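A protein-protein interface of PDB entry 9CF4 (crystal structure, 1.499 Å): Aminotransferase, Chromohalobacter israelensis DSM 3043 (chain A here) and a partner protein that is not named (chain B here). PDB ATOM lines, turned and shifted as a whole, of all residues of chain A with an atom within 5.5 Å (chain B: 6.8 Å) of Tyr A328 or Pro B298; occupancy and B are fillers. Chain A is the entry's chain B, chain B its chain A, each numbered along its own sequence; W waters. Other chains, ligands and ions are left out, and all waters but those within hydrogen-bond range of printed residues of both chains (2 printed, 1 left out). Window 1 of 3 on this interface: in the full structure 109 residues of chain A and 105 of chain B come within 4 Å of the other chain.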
ATOM      1  N   TYR A  83      -2.892 -22.125   9.277  1.00  0.00           N
ATOM      2  CA  TYR A  83      -3.737 -21.554  10.314  1.00  0.00           C
ATOM      3  C   TYR A  83      -4.155 -22.585  11.352  1.00  0.00           C
ATOM      4  O   TYR A  83      -4.581 -23.688  11.014  1.00  0.00           O
ATOM      5  CB  TYR A  83      -5.027 -20.948   9.728  1.00  0.00           C
ATOM      6  CG  TYR A  83      -6.066 -20.604  10.789  1.00  0.00           C
ATOM      7  CD1 TYR A  83      -6.045 -19.389  11.453  1.00  0.00           C
ATOM      8  CD2 TYR A  83      -7.070 -21.511  11.131  1.00  0.00           C
ATOM      9  CE1 TYR A  83      -6.984 -19.082  12.427  1.00  0.00           C
ATOM     10  CE2 TYR A  83      -7.999 -21.214  12.103  1.00  0.00           C
ATOM     11  CZ  TYR A  83      -7.954 -19.993  12.759  1.00  0.00           C
ATOM     12  OH  TYR A  83      -8.897 -19.711  13.713  1.00  0.00           O
ATOM     13  N   MET A 117      -5.929  -7.870  12.042  1.00  0.00           N
ATOM     14  CA  MET A 117      -5.731  -7.880  10.596  1.00  0.00           C
ATOM     15  C   MET A 117      -5.718  -6.494   9.961  1.00  0.00           C
ATOM     16  O   MET A 117      -5.288  -6.367   8.808  1.00  0.00           O
ATOM     17  CB  MET A 117      -6.826  -8.719   9.910  1.00  0.00           C
ATOM     18  CG  MET A 117      -6.707 -10.224  10.108  1.00  0.00           C
ATOM     19  SD  MET A 117      -7.097 -10.824  11.762  1.00  0.00           S
ATOM     20  CE  MET A 117      -8.786 -10.257  11.933  1.00  0.00           C
ATOM     21  N   GLN A 297       0.812  -9.540   3.748  1.00  0.00           N
ATOM     22  CA  GLN A 297      -0.290 -10.225   4.407  1.00  0.00           C
ATOM     23  C   GLN A 297      -0.987  -9.196   5.281  1.00  0.00           C
ATOM     24  O   GLN A 297      -0.334  -8.276   5.793  1.00  0.00           O
ATOM     25  CB  GLN A 297       0.200 -11.366   5.314  1.00  0.00           C
ATOM     26  CG  GLN A 297       0.759 -12.564   4.594  1.00  0.00           C
ATOM     27  CD  GLN A 297      -0.330 -13.431   3.986  1.00  0.00           C
ATOM     28  OE1 GLN A 297      -0.847 -14.333   4.632  1.00  0.00           O
ATOM     29  NE2 GLN A 297      -0.675 -13.157   2.725  1.00  0.00           N
ATOM     30  N   PRO A 298      -2.308  -9.308   5.453  1.00  0.00           N
ATOM     31  CA  PRO A 298      -3.005  -8.428   6.406  1.00  0.00           C
ATOM     32  C   PRO A 298      -2.615  -8.804   7.823  1.00  0.00           C
ATOM     33  O   PRO A 298      -2.733  -9.954   8.218  1.00  0.00           O
ATOM     34  CB  PRO A 298      -4.489  -8.721   6.156  1.00  0.00           C
ATOM     35  CG  PRO A 298      -4.560  -9.630   5.032  1.00  0.00           C
ATOM     36  CD  PRO A 298      -3.231 -10.253   4.793  1.00  0.00           C
ATOM     37  N   TRP A 326     -10.371 -12.334  17.636  1.00  0.00           N
ATOM     38  CA  TRP A 326     -10.751 -12.475  16.247  1.00  0.00           C
ATOM     39  C   TRP A 326     -10.335 -13.862  15.760  1.00  0.00           C
ATOM     40  O   TRP A 326      -9.244 -14.334  16.085  1.00  0.00           O
ATOM     41  CB  TRP A 326     -10.029 -11.484  15.340  1.00  0.00           C
ATOM     42  CG  TRP A 326      -9.803 -10.080  15.844  1.00  0.00           C
ATOM     43  CD1 TRP A 326      -8.592  -9.494  16.053  1.00  0.00           C
ATOM     44  CD2 TRP A 326     -10.788  -9.070  16.117  1.00  0.00           C
ATOM     45  NE1 TRP A 326      -8.755  -8.200  16.468  1.00  0.00           N
ATOM     46  CE2 TRP A 326     -10.092  -7.907  16.519  1.00  0.00           C
ATOM     47  CE3 TRP A 326     -12.186  -9.034  16.069  1.00  0.00           C
ATOM     48  CZ2 TRP A 326     -10.747  -6.730  16.866  1.00  0.00           C
ATOM     49  CZ3 TRP A 326     -12.843  -7.869  16.419  1.00  0.00           C
ATOM     50  CH2 TRP A 326     -12.104  -6.715  16.784  1.00  0.00           C
ATOM     51  N   THR A 327     -11.175 -14.484  14.934  1.00  0.00           N
ATOM     52  CA  THR A 327     -10.895 -15.847  14.471  1.00  0.00           C
ATOM     53  C   THR A 327      -9.491 -15.976  13.903  1.00  0.00           C
ATOM     54  O   THR A 327      -8.789 -16.958  14.173  1.00  0.00           O
ATOM     55  CB  THR A 327     -11.888 -16.218  13.376  1.00  0.00           C
ATOM     56  OG1 THR A 327     -13.203 -16.149  13.892  1.00  0.00           O
ATOM     57  CG2 THR A 327     -11.656 -17.609  12.829  1.00  0.00           C
ATOM     58  N   TYR A 328      -9.055 -14.976  13.129  1.00  0.00           N
ATOM     59  CA  TYR A 328      -7.771 -15.037  12.433  1.00  0.00           C
ATOM     60  C   TYR A 328      -6.629 -14.382  13.192  1.00  0.00           C
ATOM     61  O   TYR A 328      -5.525 -14.238  12.647  1.00  0.00           O
ATOM     62  CB  TYR A 328      -7.920 -14.456  11.027  1.00  0.00           C
ATOM     63  CG  TYR A 328      -8.903 -15.206  10.143  1.00  0.00           C
ATOM     64  CD1 TYR A 328      -8.981 -16.578  10.171  1.00  0.00           C
ATOM     65  CD2 TYR A 328      -9.752 -14.520   9.288  1.00  0.00           C
ATOM     66  CE1 TYR A 328      -9.870 -17.260   9.369  1.00  0.00           C
ATOM     67  CE2 TYR A 328     -10.665 -15.192   8.469  1.00  0.00           C
ATOM     68  CZ  TYR A 328     -10.700 -16.571   8.517  1.00  0.00           C
ATOM     69  OH  TYR A 328     -11.550 -17.286   7.712  1.00  0.00           O
ATOM     70  N   SER A 329      -6.854 -13.986  14.443  1.00  0.00           N
ATOM     71  CA  SER A 329      -5.785 -13.416  15.254  1.00  0.00           C
ATOM     72  C   SER A 329      -4.566 -14.333  15.277  1.00  0.00           C
ATOM     73  O   SER A 329      -4.663 -15.517  15.597  1.00  0.00           O
ATOM     74  CB  SER A 329      -6.296 -13.204  16.678  1.00  0.00           C
ATOM     75  OG  SER A 329      -5.259 -12.724  17.523  1.00  0.00           O
ATOM     76  N   GLY A 330      -3.410 -13.770  14.939  1.00  0.00           N
ATOM     77  CA  GLY A 330      -2.175 -14.505  15.003  1.00  0.00           C
ATOM     78  C   GLY A 330      -1.915 -15.419  13.834  1.00  0.00           C
ATOM     79  O   GLY A 330      -1.029 -16.267  13.936  1.00  0.00           O
ATOM     80  N   HIS A 331      -2.644 -15.259  12.735  1.00  0.00           N
ATOM     81  CA  HIS A 331      -2.521 -16.120  11.559  1.00  0.00           C
ATOM     82  C   HIS A 331      -1.073 -16.382  11.174  1.00  0.00           C
ATOM     83  O   HIS A 331      -0.291 -15.455  10.978  1.00  0.00           O
ATOM     84  CB  HIS A 331      -3.253 -15.431  10.405  1.00  0.00           C
ATOM     85  CG  HIS A 331      -3.578 -16.327   9.260  1.00  0.00           C
ATOM     86  ND1 HIS A 331      -2.652 -16.679   8.302  1.00  0.00           N
ATOM     87  CD2 HIS A 331      -4.735 -16.937   8.912  1.00  0.00           C
ATOM     88  CE1 HIS A 331      -3.215 -17.497   7.431  1.00  0.00           C
ATOM     89  NE2 HIS A 331      -4.485 -17.658   7.769  1.00  0.00           N
ATOM     90  N   LEU B  58     -11.934 -22.765  14.242  1.00  0.00           N
ATOM     91  CA  LEU B  58     -13.134 -22.146  14.807  1.00  0.00           C
ATOM     92  C   LEU B  58     -14.167 -22.114  13.678  1.00  0.00           C
ATOM     93  O   LEU B  58     -14.376 -21.083  13.036  1.00  0.00           O
ATOM     94  CB  LEU B  58     -12.825 -20.742  15.353  1.00  0.00           C
ATOM     95  CG  LEU B  58     -11.865 -20.713  16.547  1.00  0.00           C
ATOM     96  CD1 LEU B  58     -11.403 -19.288  16.837  1.00  0.00           C
ATOM     97  CD2 LEU B  58     -12.543 -21.324  17.781  1.00  0.00           C
ATOM     98  N   CYS B  60     -13.987 -23.133  10.744  1.00  0.00           N
ATOM     99  CA  CYS B  60     -13.469 -22.439   9.575  1.00  0.00           C
ATOM    100  C   CYS B  60     -12.520 -23.215   8.666  1.00  0.00           C
ATOM    101  O   CYS B  60     -12.411 -22.824   7.499  1.00  0.00           O
ATOM    102  CB  CYS B  60     -12.817 -21.101   9.969  1.00  0.00           C
ATOM    103  SG  CYS B  60     -11.440 -21.202  11.145  1.00  0.00           S
ATOM    104  N   GLY B 116     -13.399  -7.334   3.405  1.00  0.00           N
ATOM    105  CA  GLY B 116     -12.589  -7.064   4.574  1.00  0.00           C
ATOM    106  C   GLY B 116     -11.782  -8.285   4.969  1.00  0.00           C
ATOM    107  O   GLY B 116     -11.478  -9.139   4.124  1.00  0.00           O
ATOM    108  N   MET B 117     -11.444  -8.388   6.260  1.00  0.00           N
ATOM    109  CA  MET B 117     -10.529  -9.406   6.749  1.00  0.00           C
ATOM    110  C   MET B 117     -11.083 -10.270   7.870  1.00  0.00           C
ATOM    111  O   MET B 117     -10.471 -11.301   8.187  1.00  0.00           O
ATOM    112  CB  MET B 117      -9.222  -8.758   7.244  1.00  0.00           C
ATOM    113  CG  MET B 117      -8.323  -8.239   6.121  1.00  0.00           C
ATOM    114  SD  MET B 117      -8.881  -6.728   5.309  1.00  0.00           S
ATOM    115  CE  MET B 117      -9.003  -5.602   6.691  1.00  0.00           C
ATOM    116  N   SER B 118     -12.191  -9.876   8.493  1.00  0.00           N
ATOM    117  CA  SER B 118     -12.773 -10.631   9.587  1.00  0.00           C
ATOM    118  C   SER B 118     -14.291 -10.493   9.532  1.00  0.00           C
ATOM    119  O   SER B 118     -14.834  -9.526   8.985  1.00  0.00           O
ATOM    120  CB  SER B 118     -12.272 -10.084  10.922  1.00  0.00           C
ATOM    121  OG  SER B 118     -12.725  -8.734  11.130  1.00  0.00           O
ATOM    122  N   GLY B 119     -14.987 -11.470  10.109  1.00  0.00           N
ATOM    123  CA  GLY B 119     -16.428 -11.318  10.255  1.00  0.00           C
ATOM    124  C   GLY B 119     -16.805 -10.091  11.062  1.00  0.00           C
ATOM    125  O   GLY B 119     -17.836  -9.459  10.812  1.00  0.00           O
ATOM    126  N   ALA B 289     -17.352 -14.864   6.101  1.00  0.00           N
ATOM    127  CA  ALA B 289     -15.932 -15.011   6.383  1.00  0.00           C
ATOM    128  C   ALA B 289     -15.656 -16.514   6.518  1.00  0.00           C
ATOM    129  O   ALA B 289     -16.229 -17.314   5.773  1.00  0.00           O
ATOM    130  CB  ALA B 289     -15.524 -14.198   7.609  1.00  0.00           C
ATOM    131  N1  LLP B 290     -20.243 -13.699  13.029  1.00  0.00           N
ATOM    132  C2  LLP B 290     -20.341 -14.974  13.272  1.00  0.00           C
ATOM    133  C2' LLP B 290     -21.652 -15.644  13.119  1.00  0.00           C
ATOM    134  C3  LLP B 290     -19.206 -15.695  13.647  1.00  0.00           C
ATOM    135  O3  LLP B 290     -19.219 -16.997  13.940  1.00  0.00           O
ATOM    136  C4  LLP B 290     -18.003 -15.041  13.753  1.00  0.00           C
ATOM    137  C4' LLP B 290     -16.817 -15.835  14.140  1.00  0.00           C
ATOM    138  C5  LLP B 290     -17.916 -13.692  13.489  1.00  0.00           C
ATOM    139  C6  LLP B 290     -19.080 -13.035  13.139  1.00  0.00           C
ATOM    140  C5' LLP B 290     -16.618 -12.928  13.648  1.00  0.00           C
ATOM    141  OP4 LLP B 290     -15.762 -13.226  12.657  1.00  0.00           O
ATOM    142  P   LLP B 290     -14.187 -12.996  13.262  1.00  0.00           P
ATOM    143  OP1 LLP B 290     -13.456 -13.154  11.962  1.00  0.00           O
ATOM    144  OP2 LLP B 290     -13.911 -11.449  13.612  1.00  0.00           O
ATOM    145  OP3 LLP B 290     -13.329 -13.590  14.487  1.00  0.00           O
ATOM    146  N   LLP B 290     -14.766 -16.912   7.432  1.00  0.00           N
ATOM    147  CA  LLP B 290     -14.491 -18.322   7.742  1.00  0.00           C
ATOM    148  CB  LLP B 290     -15.445 -18.844   8.822  1.00  0.00           C
ATOM    149  CG  LLP B 290     -15.293 -18.120  10.206  1.00  0.00           C
ATOM    150  CD  LLP B 290     -16.097 -18.761  11.332  1.00  0.00           C
ATOM    151  CE  LLP B 290     -15.696 -18.244  12.749  1.00  0.00           C
ATOM    152  NZ  LLP B 290     -16.537 -17.112  13.343  1.00  0.00           N
ATOM    153  C   LLP B 290     -14.405 -19.251   6.529  1.00  0.00           C
ATOM    154  O   LLP B 290     -13.353 -19.325   5.876  1.00  0.00           O
ATOM    155  N   GLY B 291     -15.478 -19.984   6.233  1.00  0.00           N
ATOM    156  CA  GLY B 291     -15.491 -20.935   5.125  1.00  0.00           C
ATOM    157  C   GLY B 291     -15.313 -20.314   3.759  1.00  0.00           C
ATOM    158  O   GLY B 291     -15.147 -21.055   2.780  1.00  0.00           O
ATOM    159  N   LEU B 292     -15.309 -18.974   3.667  1.00  0.00           N
ATOM    160  CA  LEU B 292     -14.992 -18.313   2.401  1.00  0.00           C
ATOM    161  C   LEU B 292     -13.590 -18.660   1.908  1.00  0.00           C
ATOM    162  O   LEU B 292     -13.376 -18.803   0.699  1.00  0.00           O
ATOM    163  CB  LEU B 292     -15.139 -16.798   2.586  1.00  0.00           C
ATOM    164  CG  LEU B 292     -14.700 -15.903   1.436  1.00  0.00           C
ATOM    165  CD1 LEU B 292     -15.465 -16.222   0.143  1.00  0.00           C
ATOM    166  CD2 LEU B 292     -14.878 -14.448   1.835  1.00  0.00           C
ATOM    167  N   THR B 293     -12.612 -18.765   2.819  1.00  0.00           N
ATOM    168  CA  THR B 293     -11.255 -19.149   2.455  1.00  0.00           C
ATOM    169  C   THR B 293     -10.771 -20.384   3.202  1.00  0.00           C
ATOM    170  O   THR B 293      -9.591 -20.731   3.086  1.00  0.00           O
ATOM    171  CB  THR B 293     -10.257 -18.042   2.786  1.00  0.00           C
ATOM    172  OG1 THR B 293     -10.354 -17.760   4.193  1.00  0.00           O
ATOM    173  CG2 THR B 293     -10.503 -16.803   1.978  1.00  0.00           C
ATOM    174  N   SER B 294     -11.616 -20.999   4.033  1.00  0.00           N
ATOM    175  CA  SER B 294     -11.191 -22.076   4.933  1.00  0.00           C
ATOM    176  C   SER B 294     -10.018 -21.653   5.803  1.00  0.00           C
ATOM    177  O   SER B 294      -9.202 -22.480   6.205  1.00  0.00           O
ATOM    178  CB  SER B 294     -10.916 -23.385   4.193  1.00  0.00           C
ATOM    179  OG  SER B 294     -12.144 -24.000   3.821  1.00  0.00           O
ATOM    180  N   ALA B 295      -9.954 -20.359   6.099  1.00  0.00           N
ATOM    181  CA  ALA B 295      -8.946 -19.748   6.964  1.00  0.00           C
ATOM    182  C   ALA B 295      -7.548 -19.718   6.360  1.00  0.00           C
ATOM    183  O   ALA B 295      -6.595 -19.295   7.049  1.00  0.00           O
ATOM    184  CB  ALA B 295      -8.907 -20.379   8.363  1.00  0.00           C
ATOM    185  N   TYR B 296      -7.379 -20.100   5.087  1.00  0.00           N
ATOM    186  CA  TYR B 296      -6.035 -20.080   4.502  1.00  0.00           C
ATOM    187  C   TYR B 296      -5.517 -18.657   4.372  1.00  0.00           C
ATOM    188  O   TYR B 296      -4.304 -18.448   4.404  1.00  0.00           O
ATOM    189  CB  TYR B 296      -5.991 -20.865   3.183  1.00  0.00           C
ATOM    190  CG  TYR B 296      -5.923 -22.354   3.409  1.00  0.00           C
ATOM    191  CD1 TYR B 296      -4.710 -22.983   3.591  1.00  0.00           C
ATOM    192  CD2 TYR B 296      -7.059 -23.120   3.533  1.00  0.00           C
ATOM    193  CE1 TYR B 296      -4.627 -24.313   3.824  1.00  0.00           C
ATOM    194  CE2 TYR B 296      -6.975 -24.482   3.792  1.00  0.00           C
ATOM    195  CZ  TYR B 296      -5.759 -25.062   3.951  1.00  0.00           C
ATOM    196  OH  TYR B 296      -5.622 -26.403   4.226  1.00  0.00           O
ATOM    197  N   GLN B 297      -6.413 -17.686   4.208  1.00  0.00           N
ATOM    198  CA  GLN B 297      -6.099 -16.268   4.284  1.00  0.00           C
ATOM    199  C   GLN B 297      -7.235 -15.578   5.025  1.00  0.00           C
ATOM    200  O   GLN B 297      -8.384 -16.002   4.915  1.00  0.00           O
ATOM    201  CB  GLN B 297      -6.007 -15.648   2.879  1.00  0.00           C
ATOM    202  CG  GLN B 297      -4.808 -16.109   2.040  1.00  0.00           C
ATOM    203  CD  GLN B 297      -3.544 -15.453   2.484  1.00  0.00           C
ATOM    204  OE1 GLN B 297      -3.204 -14.367   2.012  1.00  0.00           O
ATOM    205  NE2 GLN B 297      -2.833 -16.092   3.406  1.00  0.00           N
ATOM    206  N   PRO B 298      -6.960 -14.488   5.734  1.00  0.00           N
ATOM    207  CA  PRO B 298      -8.054 -13.720   6.351  1.00  0.00           C
ATOM    208  C   PRO B 298      -8.815 -12.951   5.279  1.00  0.00           C
ATOM    209  O   PRO B 298      -8.246 -12.125   4.578  1.00  0.00           O
ATOM    210  CB  PRO B 298      -7.332 -12.768   7.316  1.00  0.00           C
ATOM    211  CG  PRO B 298      -5.898 -13.074   7.224  1.00  0.00           C
ATOM    212  CD  PRO B 298      -5.630 -13.928   6.059  1.00  0.00           C
ATOM    213  N   LEU B 299     -10.104 -13.216   5.162  1.00  0.00           N
ATOM    214  CA  LEU B 299     -10.947 -12.536   4.194  1.00  0.00           C
ATOM    215  C   LEU B 299     -12.378 -12.543   4.723  1.00  0.00           C
ATOM    216  O   LEU B 299     -12.858 -13.555   5.240  1.00  0.00           O
ATOM    217  CB  LEU B 299     -10.897 -13.226   2.817  1.00  0.00           C
ATOM    218  CG  LEU B 299     -11.388 -12.399   1.616  1.00  0.00           C
ATOM    219  CD1 LEU B 299     -10.384 -11.293   1.326  1.00  0.00           C
ATOM    220  CD2 LEU B 299     -11.600 -13.255   0.392  1.00  0.00           C
ATOM    221  N   SER B 300     -13.070 -11.425   4.555  1.00  0.00           N
ATOM    222  CA  SER B 300     -14.490 -11.327   4.877  1.00  0.00           C
ATOM    223  C   SER B 300     -15.200 -10.632   3.733  1.00  0.00           C
ATOM    224  O   SER B 300     -14.579  -9.991   2.876  1.00  0.00           O
ATOM    225  CB  SER B 300     -14.729 -10.531   6.164  1.00  0.00           C
ATOM    226  OG  SER B 300     -14.549  -9.161   5.911  1.00  0.00           O
ATOM    227  N   TYR B 328      -6.354  -3.085   3.479  1.00  0.00           N
ATOM    228  CA  TYR B 328      -6.179  -4.400   2.877  1.00  0.00           C
ATOM    229  C   TYR B 328      -7.448  -4.955   2.230  1.00  0.00           C
ATOM    230  O   TYR B 328      -7.454  -6.139   1.847  1.00  0.00           O
ATOM    231  CB  TYR B 328      -5.625  -5.386   3.906  1.00  0.00           C
ATOM    232  CG  TYR B 328      -4.278  -4.988   4.510  1.00  0.00           C
ATOM    233  CD1 TYR B 328      -3.291  -4.418   3.710  1.00  0.00           C
ATOM    234  CD2 TYR B 328      -3.993  -5.179   5.849  1.00  0.00           C
ATOM    235  CE1 TYR B 328      -2.081  -4.056   4.215  1.00  0.00           C
ATOM    236  CE2 TYR B 328      -2.752  -4.801   6.384  1.00  0.00           C
ATOM    237  CZ  TYR B 328      -1.796  -4.250   5.537  1.00  0.00           C
ATOM    238  OH  TYR B 328      -0.531  -3.898   5.989  1.00  0.00           O
ATOM    239  N   HIS B 331      -7.522  -7.788  -0.763  1.00  0.00           N
ATOM    240  CA  HIS B 331      -6.152  -8.281  -0.873  1.00  0.00           C
ATOM    241  C   HIS B 331      -6.070  -9.438  -1.854  1.00  0.00           C
ATOM    242  O   HIS B 331      -6.788 -10.431  -1.721  1.00  0.00           O
ATOM    243  CB  HIS B 331      -5.694  -8.733   0.518  1.00  0.00           C
ATOM    244  CG  HIS B 331      -4.215  -8.890   0.650  1.00  0.00           C
ATOM    245  ND1 HIS B 331      -3.534  -9.992   0.170  1.00  0.00           N
ATOM    246  CD2 HIS B 331      -3.283  -8.068   1.181  1.00  0.00           C
ATOM    247  CE1 HIS B 331      -2.244  -9.835   0.414  1.00  0.00           C
ATOM    248  NE2 HIS B 331      -2.072  -8.690   1.047  1.00  0.00           N
ATOM    249  N   GLY B 334      -5.605 -12.947  -0.500  1.00  0.00           N
ATOM    250  CA  GLY B 334      -6.841 -13.415   0.110  1.00  0.00           C
ATOM    251  C   GLY B 334      -7.852 -13.876  -0.917  1.00  0.00           C
ATOM    252  O   GLY B 334      -8.470 -14.946  -0.776  1.00  0.00           O
ATOM    253  N   CYS B 335      -8.010 -13.102  -1.985  1.00  0.00           N
ATOM    254  CA  CYS B 335      -8.965 -13.471  -3.021  1.00  0.00           C
ATOM    255  C   CYS B 335      -8.508 -14.694  -3.805  1.00  0.00           C
ATOM    256  O   CYS B 335      -9.330 -15.552  -4.157  1.00  0.00           O
ATOM    257  CB  CYS B 335      -9.218 -12.278  -3.930  1.00  0.00           C
ATOM    258  SG  CYS B 335     -10.070 -10.906  -3.096  1.00  0.00           S
HETATM  259  O   HOH W   1     -12.353 -16.150   5.389  1.00  0.00           O
HETATM  260  O   HOH W   2     -10.893 -12.997  12.009  1.00  0.00           O
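OP1 of LLP B290 sits at hydrogen-bond distance from the backbone NH of Gly B119 (2.9 Å).
The backbone NH (N) of Met B117 is in hydrogen-bond range of the side-chain hydroxyl (OG) of Ser B300.
O of Leu B58 lies close to SG of Cys B60 (3.5 Å).
The side-chain hydroxyl of Tyr A83 is in hydrogen-bond range of the backbone carbonyl oxygen of Thr A327 (2.8 Å).
OG1 of Thr B293 is in hydrogen-bond range of O of Gln B297.
The side-chain hydroxyl (OG) of Ser B300 lies close to the backbone carbonyl oxygen (O) of Ser B118 (3.1 Å).
A ring nitrogen (NE2) of His A331 lies close to the backbone carbonyl oxygen of Tyr B296 (3.5 Å).
OP3 of LLP B290 sits at hydrogen-bond distance from OG1 of Thr A327, at 2.6 Å.
A ring nitrogen (NE2) of His A331 sits at hydrogen-bond distance from the backbone carbonyl oxygen (O) of Ala B295.
OH of Tyr A328 lies close to N of LLP B290.
The side-chain amide oxygen of Gln B297 sits at hydrogen-bond distance from the side-chain amide nitrogen of Gln A297 (2.9 Å).
Printed residues of chain B within 4 Å of Tyr A328: Met B117, LLP B290, Thr B293, Ala B295, Pro B298 and Leu B299.
Printed residues of chain A within 4 Å of Pro B298: Met A117 (3.8 Å) and Tyr A328 (3.5 Å).
Printed residues of chain B within 4 Å of Gln A297: Gln B297 (2.9 Å).
Of the printed residues of chain A, Leu B299 touches Tyr A328.
Of the printed residues of chain B, Pro A298 touches Met B117 (3.9 Å) and Tyr B328 (3.4 Å).
The nearest printed residue of chain A that does not touch Pro B298 is His A331 (4.2 Å).
Of the 22 printed residues of chain B, 11 touch a printed residue of chain A.
Hydrophobic or aromatic side chains of chain B that line the printed part of chain A: Met B117, Ala B295, Pro B298 and Tyr B328.
Of the 10 printed residues of chain A, 8 touch a printed residue of chain B.
Among the printed residues, no Asp or Glu carboxylate lies within 4 Å of a Lys or Arg side-chain nitrogen of the other chain.
Water W2 lies within hydrogen-bond range of OP1 of LLP B290, N of Tyr A328 and N of Thr A327.
Water W1 lies within hydrogen-bond range of the backbone carbonyl oxygen (O) of Leu B299 (2.6 Å), the side-chain hydroxyl (OH) of Tyr A328 (2.7 Å), the side-chain hydroxyl (OG1) of Thr B293 (2.8 Å) and N of LLP B290 (3.3 Å).
Ala B295 touches Tyr A83.
Met A117 touches Met B117 (CB to CB, 3.6 Å).
Met A117 touches Pro B298.
Tyr B328 touches Met A117 (CD2 to O, 3.4 Å).
CD2 of Tyr B328 touches CA of Pro A298, 3.4 Å away.
SG of Cys B60 touches CG2 of Thr A327 (3.97 Å).
Tyr A328 touches Met B117 (CD2 to O, 3.5 Å).
OG1 of Thr B293 touches OH of Tyr A328 (3.7 Å).
CE1 of Tyr A328 touches CB of Ala B295, at 3.4 Å.
CE2 of Tyr A328 touches N of Leu B299 (3.9 Å).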
